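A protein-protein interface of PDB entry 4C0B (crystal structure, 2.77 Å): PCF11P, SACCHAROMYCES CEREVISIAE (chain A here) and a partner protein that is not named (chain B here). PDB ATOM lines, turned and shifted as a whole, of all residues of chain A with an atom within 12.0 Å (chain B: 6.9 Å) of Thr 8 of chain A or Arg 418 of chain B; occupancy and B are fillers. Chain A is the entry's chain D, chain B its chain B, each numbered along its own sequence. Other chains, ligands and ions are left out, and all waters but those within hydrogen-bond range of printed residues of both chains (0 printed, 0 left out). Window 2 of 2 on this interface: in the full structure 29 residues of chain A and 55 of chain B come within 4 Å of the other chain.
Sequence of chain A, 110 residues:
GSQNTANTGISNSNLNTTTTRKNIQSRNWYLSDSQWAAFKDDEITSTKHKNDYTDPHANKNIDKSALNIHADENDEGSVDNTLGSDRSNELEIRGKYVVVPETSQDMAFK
NH2 of Arg 422 of chain B sits at hydrogen-bond distance from O of Ser 11 of chain A (2.8 Å).
NE of Arg 422 of chain B is in hydrogen-bond range of OD1 of Asn 12 of chain A (2.8 Å).
The guanidinium group (NH1) of Arg 418 of chain B lies within hydrogen-bond range of the side-chain hydroxyl (OG1) of Thr 8 of chain A (3.1 Å).
OD1 of Asp 349 of chain B is in salt-bridge range of NZ of Lys 420 of chain B (3.0 Å).
The backbone carbonyl oxygen (O) of Lys 420 of chain B sits at hydrogen-bond distance from the backbone NH (N) of Asn 415 of chain B (2.9 Å).
The side-chain amide oxygen (OD1) of Asn 415 of chain B lies within hydrogen-bond range of the backbone NH (N) of Lys 417 of chain B (3.4 Å).
OD1 of Asn 415 of chain B is in hydrogen-bond range of N of Arg 418 of chain B, 2.9 Å away.
O of Glu 413 of chain B sits at hydrogen-bond distance from N of Arg 422 of chain B, at 2.8 Å.
CB of Glu 413 of chain B touches CA of Asn 7 of chain A, 3.5 Å away.
Asn 7 of chain A touches Asn 415 of chain B (N to ND2, 3.6 Å).
Asn 7 of chain A touches Arg 418 of chain B.
ND2 of Asn 7 of chain A touches CB of Lys 420 of chain B, at 3.3 Å.
Arg 422 of chain B touches Asn 7 of chain A.
Arg 422 of chain B touches Ile 10 of chain A.
Arg 422 of chain B touches Leu 15 of chain A.
Thr 8 of chain A touches just one residue of chain B: Arg 418.
Of the printed residues of chain B, Ile 10 of chain A touches Arg 422.
Printed residues of chain B within 4 Å of Ser 11 of chain A: Arg 422.
Of chain A, only Asn 7 (3.5 Å) comes within 4 Å of Glu 413 of chain B.
Of chain A, only Asn 7 and Thr 8 come within 4 Å of Arg 418 of chain B.
Lys 420 of chain B touches just one residue of chain A: Asn 7.
Of the printed residues of chain A, Arg 422 of chain B touches Asn 7, Ile 10, Ser 11, Asn 12 and Leu 15.
Of the 11 printed residues of chain B, 5 touch a printed residue of chain A.
Among the printed residues, no Asp or Glu carboxylate lies within 4 Å of a Lys or Arg side-chain nitrogen of the other chain.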
ATOM      1  N   ASN A   7      20.698   0.866   2.120  1.00  0.00           N
ATOM      2  CA  ASN A   7      20.869  -0.501   2.620  1.00  0.00           C
ATOM      3  C   ASN A   7      20.410  -0.645   4.083  1.00  0.00           C
ATOM      4  O   ASN A   7      19.490  -1.422   4.358  1.00  0.00           O
ATOM      5  CB  ASN A   7      22.320  -0.969   2.443  1.00  0.00           C
ATOM      6  CG  ASN A   7      22.557  -2.429   2.742  1.00  0.00           C
ATOM      7  OD1 ASN A   7      22.303  -2.936   3.841  1.00  0.00           O
ATOM      8  ND2 ASN A   7      23.115  -3.124   1.784  1.00  0.00           N
ATOM      9  N   THR A   8      21.053   0.109   5.013  1.00  0.00           N
ATOM     10  CA  THR A   8      20.787   0.100   6.462  1.00  0.00           C
ATOM     11  C   THR A   8      19.360   0.593   6.867  1.00  0.00           C
ATOM     12  O   THR A   8      19.155   1.005   8.013  1.00  0.00           O
ATOM     13  CB  THR A   8      21.989   0.729   7.245  1.00  0.00           C
ATOM     14  OG1 THR A   8      22.581   1.792   6.487  1.00  0.00           O
ATOM     15  CG2 THR A   8      23.067  -0.297   7.598  1.00  0.00           C
ATOM     16  N   GLY A   9      18.403   0.491   5.933  1.00  0.00           N
ATOM     17  CA  GLY A   9      17.003   0.896   6.067  1.00  0.00           C
ATOM     18  C   GLY A   9      16.245   0.284   7.229  1.00  0.00           C
ATOM     19  O   GLY A   9      15.513   0.997   7.928  1.00  0.00           O
ATOM     20  N   ILE A  10      16.419  -1.041   7.443  1.00  0.00           N
ATOM     21  CA  ILE A  10      15.800  -1.802   8.541  1.00  0.00           C
ATOM     22  C   ILE A  10      16.773  -2.894   9.099  1.00  0.00           C
ATOM     23  O   ILE A  10      17.988  -2.795   8.874  1.00  0.00           O
ATOM     24  CB  ILE A  10      14.329  -2.279   8.190  1.00  0.00           C
ATOM     25  CG1 ILE A  10      13.454  -2.600   9.455  1.00  0.00           C
ATOM     26  CG2 ILE A  10      14.286  -3.372   7.108  1.00  0.00           C
ATOM     27  CD1 ILE A  10      11.964  -3.061   9.211  1.00  0.00           C
ATOM     28  N   SER A  11      16.238  -3.909   9.827  1.00  0.00           N
ATOM     29  CA  SER A  11      16.964  -5.019  10.451  1.00  0.00           C
ATOM     30  C   SER A  11      17.245  -6.223   9.543  1.00  0.00           C
ATOM     31  O   SER A  11      16.351  -6.743   8.871  1.00  0.00           O
ATOM     32  CB  SER A  11      16.244  -5.497  11.714  1.00  0.00           C
ATOM     33  OG  SER A  11      15.111  -6.308  11.432  1.00  0.00           O
ATOM     34  N   ASN A  12      18.510  -6.651   9.562  1.00  0.00           N
ATOM     35  CA  ASN A  12      19.071  -7.854   8.949  1.00  0.00           C
ATOM     36  C   ASN A  12      19.309  -8.721  10.216  1.00  0.00           C
ATOM     37  O   ASN A  12      19.571  -8.142  11.270  1.00  0.00           O
ATOM     38  CB  ASN A  12      20.407  -7.532   8.200  1.00  0.00           C
ATOM     39  CG  ASN A  12      20.306  -6.531   7.050  1.00  0.00           C
ATOM     40  OD1 ASN A  12      19.395  -5.697   6.975  1.00  0.00           O
ATOM     41  ND2 ASN A  12      21.256  -6.549   6.135  1.00  0.00           N
ATOM     42  N   SER A  13      19.111 -10.040  10.212  1.00  0.00           N
ATOM     43  CA  SER A  13      18.852 -10.906   9.085  1.00  0.00           C
ATOM     44  C   SER A  13      17.487 -11.647   9.137  1.00  0.00           C
ATOM     45  O   SER A  13      16.677 -11.363   8.263  1.00  0.00           O
ATOM     46  CB  SER A  13      20.050 -11.824   8.857  1.00  0.00           C
ATOM     47  OG  SER A  13      21.309 -11.155   8.873  1.00  0.00           O
ATOM     48  N   LEU A  15      13.701 -12.240   9.712  1.00  0.00           N
ATOM     49  CA  LEU A  15      12.539 -11.358   9.824  1.00  0.00           C
ATOM     50  C   LEU A  15      11.276 -12.062  10.385  1.00  0.00           C
ATOM     51  O   LEU A  15      11.086 -13.257  10.142  1.00  0.00           O
ATOM     52  CB  LEU A  15      12.305 -10.682   8.459  1.00  0.00           C
ATOM     53  CG  LEU A  15      12.996  -9.321   8.216  1.00  0.00           C
ATOM     54  CD1 LEU A  15      14.501  -9.361   8.406  1.00  0.00           C
ATOM     55  CD2 LEU A  15      12.732  -8.831   6.854  1.00  0.00           C
ATOM     56  N   ASP B 349      27.246  -6.966  -1.779  1.00  0.00           N
ATOM     57  CA  ASP B 349      28.043  -6.011  -2.546  1.00  0.00           C
ATOM     58  C   ASP B 349      27.621  -6.061  -4.007  1.00  0.00           C
ATOM     59  O   ASP B 349      27.229  -7.123  -4.480  1.00  0.00           O
ATOM     60  CB  ASP B 349      29.533  -6.349  -2.450  1.00  0.00           C
ATOM     61  CG  ASP B 349      30.243  -5.662  -1.305  1.00  0.00           C
ATOM     62  OD1 ASP B 349      30.450  -4.424  -1.390  1.00  0.00           O
ATOM     63  OD2 ASP B 349      30.623  -6.364  -0.336  1.00  0.00           O
ATOM     64  N   TYR B 350      27.734  -4.925  -4.729  1.00  0.00           N
ATOM     65  CA  TYR B 350      27.425  -4.780  -6.165  1.00  0.00           C
ATOM     66  C   TYR B 350      28.084  -5.917  -6.988  1.00  0.00           C
ATOM     67  O   TYR B 350      27.454  -6.519  -7.857  1.00  0.00           O
ATOM     68  CB  TYR B 350      27.973  -3.412  -6.655  1.00  0.00           C
ATOM     69  CG  TYR B 350      26.995  -2.253  -6.700  1.00  0.00           C
ATOM     70  CD1 TYR B 350      26.033  -2.079  -5.701  1.00  0.00           C
ATOM     71  CD2 TYR B 350      27.069  -1.292  -7.705  1.00  0.00           C
ATOM     72  CE1 TYR B 350      25.148  -0.996  -5.728  1.00  0.00           C
ATOM     73  CE2 TYR B 350      26.187  -0.211  -7.746  1.00  0.00           C
ATOM     74  CZ  TYR B 350      25.233  -0.061  -6.752  1.00  0.00           C
ATOM     75  OH  TYR B 350      24.381   1.016  -6.794  1.00  0.00           O
ATOM     76  N   GLU B 351      29.340  -6.225  -6.650  1.00  0.00           N
ATOM     77  CA  GLU B 351      30.228  -7.235  -7.233  1.00  0.00           C
ATOM     78  C   GLU B 351      29.701  -8.687  -7.104  1.00  0.00           C
ATOM     79  O   GLU B 351      30.094  -9.539  -7.893  1.00  0.00           O
ATOM     80  CB  GLU B 351      31.627  -7.141  -6.570  1.00  0.00           C
ATOM     81  CG  GLU B 351      32.402  -5.837  -6.784  1.00  0.00           C
ATOM     82  CD  GLU B 351      31.912  -4.566  -6.087  1.00  0.00           C
ATOM     83  OE1 GLU B 351      31.003  -4.629  -5.223  1.00  0.00           O
ATOM     84  OE2 GLU B 351      32.503  -3.500  -6.363  1.00  0.00           O
ATOM     85  N   GLU B 413      16.722  -2.504  -0.762  1.00  0.00           N
ATOM     86  CA  GLU B 413      17.515  -1.275  -0.862  1.00  0.00           C
ATOM     87  C   GLU B 413      18.705  -1.457  -1.799  1.00  0.00           C
ATOM     88  O   GLU B 413      19.274  -2.543  -1.866  1.00  0.00           O
ATOM     89  CB  GLU B 413      18.074  -0.837   0.515  1.00  0.00           C
ATOM     90  CG  GLU B 413      17.108  -0.794   1.686  1.00  0.00           C
ATOM     91  CD  GLU B 413      16.203   0.419   1.728  1.00  0.00           C
ATOM     92  OE1 GLU B 413      16.707   1.511   2.074  1.00  0.00           O
ATOM     93  OE2 GLU B 413      14.988   0.273   1.450  1.00  0.00           O
ATOM     94  N   ASN B 415      22.137   0.909  -2.416  1.00  0.00           N
ATOM     95  CA  ASN B 415      22.946   2.017  -1.926  1.00  0.00           C
ATOM     96  C   ASN B 415      24.064   2.267  -2.931  1.00  0.00           C
ATOM     97  O   ASN B 415      24.910   1.386  -3.127  1.00  0.00           O
ATOM     98  CB  ASN B 415      23.529   1.623  -0.568  1.00  0.00           C
ATOM     99  CG  ASN B 415      24.059   2.756   0.266  1.00  0.00           C
ATOM    100  OD1 ASN B 415      24.899   3.557  -0.171  1.00  0.00           O
ATOM    101  ND2 ASN B 415      23.624   2.794   1.521  1.00  0.00           N
ATOM    102  N   GLU B 416      24.061   3.451  -3.589  1.00  0.00           N
ATOM    103  CA  GLU B 416      25.083   3.804  -4.589  1.00  0.00           C
ATOM    104  C   GLU B 416      26.393   4.167  -3.916  1.00  0.00           C
ATOM    105  O   GLU B 416      27.443   3.655  -4.307  1.00  0.00           O
ATOM    106  CB  GLU B 416      24.653   4.977  -5.490  1.00  0.00           C
ATOM    107  CG  GLU B 416      23.310   4.831  -6.176  1.00  0.00           C
ATOM    108  CD  GLU B 416      22.151   5.502  -5.458  1.00  0.00           C
ATOM    109  OE1 GLU B 416      21.774   5.039  -4.353  1.00  0.00           O
ATOM    110  OE2 GLU B 416      21.564   6.441  -6.048  1.00  0.00           O
ATOM    111  N   LYS B 417      26.319   5.067  -2.910  1.00  0.00           N
ATOM    112  CA  LYS B 417      27.451   5.603  -2.152  1.00  0.00           C
ATOM    113  C   LYS B 417      28.342   4.511  -1.557  1.00  0.00           C
ATOM    114  O   LYS B 417      29.542   4.506  -1.847  1.00  0.00           O
ATOM    115  CB  LYS B 417      27.002   6.650  -1.108  1.00  0.00           C
ATOM    116  CG  LYS B 417      26.505   7.956  -1.735  1.00  0.00           C
ATOM    117  CD  LYS B 417      26.347   9.081  -0.711  1.00  0.00           C
ATOM    118  CE  LYS B 417      26.253  10.433  -1.381  1.00  0.00           C
ATOM    119  NZ  LYS B 417      25.569  11.437  -0.525  1.00  0.00           N
ATOM    120  N   ARG B 418      27.746   3.519  -0.852  1.00  0.00           N
ATOM    121  CA  ARG B 418      28.450   2.384  -0.229  1.00  0.00           C
ATOM    122  C   ARG B 418      28.692   1.161  -1.172  1.00  0.00           C
ATOM    123  O   ARG B 418      29.526   0.311  -0.850  1.00  0.00           O
ATOM    124  CB  ARG B 418      27.696   1.915   1.034  1.00  0.00           C
ATOM    125  CG  ARG B 418      27.935   2.725   2.310  1.00  0.00           C
ATOM    126  CD  ARG B 418      26.909   2.374   3.397  1.00  0.00           C
ATOM    127  NE  ARG B 418      27.045   1.000   3.920  1.00  0.00           N
ATOM    128  CZ  ARG B 418      26.071   0.294   4.504  1.00  0.00           C
ATOM    129  NH1 ARG B 418      24.850   0.806   4.631  1.00  0.00           N
ATOM    130  NH2 ARG B 418      26.307  -0.936   4.945  1.00  0.00           N
ATOM    131  N   ARG B 419      27.959   1.074  -2.312  1.00  0.00           N
ATOM    132  CA  ARG B 419      27.962  -0.025  -3.311  1.00  0.00           C
ATOM    133  C   ARG B 419      27.485  -1.363  -2.755  1.00  0.00           C
ATOM    134  O   ARG B 419      28.070  -2.421  -3.008  1.00  0.00           O
ATOM    135  CB  ARG B 419      29.260  -0.139  -4.126  1.00  0.00           C
ATOM    136  CG  ARG B 419      29.345   0.909  -5.217  1.00  0.00           C
ATOM    137  CD  ARG B 419      30.703   0.891  -5.873  1.00  0.00           C
ATOM    138  NE  ARG B 419      30.901  -0.299  -6.706  1.00  0.00           N
ATOM    139  CZ  ARG B 419      30.529  -0.393  -7.982  1.00  0.00           C
ATOM    140  NH1 ARG B 419      29.924   0.631  -8.583  1.00  0.00           N
ATOM    141  NH2 ARG B 419      30.746  -1.512  -8.663  1.00  0.00           N
ATOM    142  N   LYS B 420      26.372  -1.293  -2.019  1.00  0.00           N
ATOM    143  CA  LYS B 420      25.742  -2.427  -1.360  1.00  0.00           C
ATOM    144  C   LYS B 420      24.245  -2.506  -1.712  1.00  0.00           C
ATOM    145  O   LYS B 420      23.655  -1.522  -2.161  1.00  0.00           O
ATOM    146  CB  LYS B 420      25.930  -2.344   0.182  1.00  0.00           C
ATOM    147  CG  LYS B 420      27.349  -2.055   0.684  1.00  0.00           C
ATOM    148  CD  LYS B 420      28.219  -3.289   0.850  1.00  0.00           C
ATOM    149  CE  LYS B 420      29.567  -2.881   1.392  1.00  0.00           C
ATOM    150  NZ  LYS B 420      30.474  -4.040   1.569  1.00  0.00           N
ATOM    151  N   ARG B 422      20.406  -4.525  -0.219  1.00  0.00           N
ATOM    152  CA  ARG B 422      19.802  -5.329   0.822  1.00  0.00           C
ATOM    153  C   ARG B 422      18.869  -6.283   0.094  1.00  0.00           C
ATOM    154  O   ARG B 422      17.976  -5.836  -0.631  1.00  0.00           O
ATOM    155  CB  ARG B 422      19.059  -4.487   1.839  1.00  0.00           C
ATOM    156  CG  ARG B 422      18.803  -5.221   3.131  1.00  0.00           C
ATOM    157  CD  ARG B 422      17.991  -4.344   4.050  1.00  0.00           C
ATOM    158  NE  ARG B 422      17.405  -5.098   5.154  1.00  0.00           N
ATOM    159  CZ  ARG B 422      16.187  -5.626   5.130  1.00  0.00           C
ATOM    160  NH1 ARG B 422      15.414  -5.484   4.063  1.00  0.00           N
ATOM    161  NH2 ARG B 422      15.728  -6.289   6.182  1.00  0.00           N
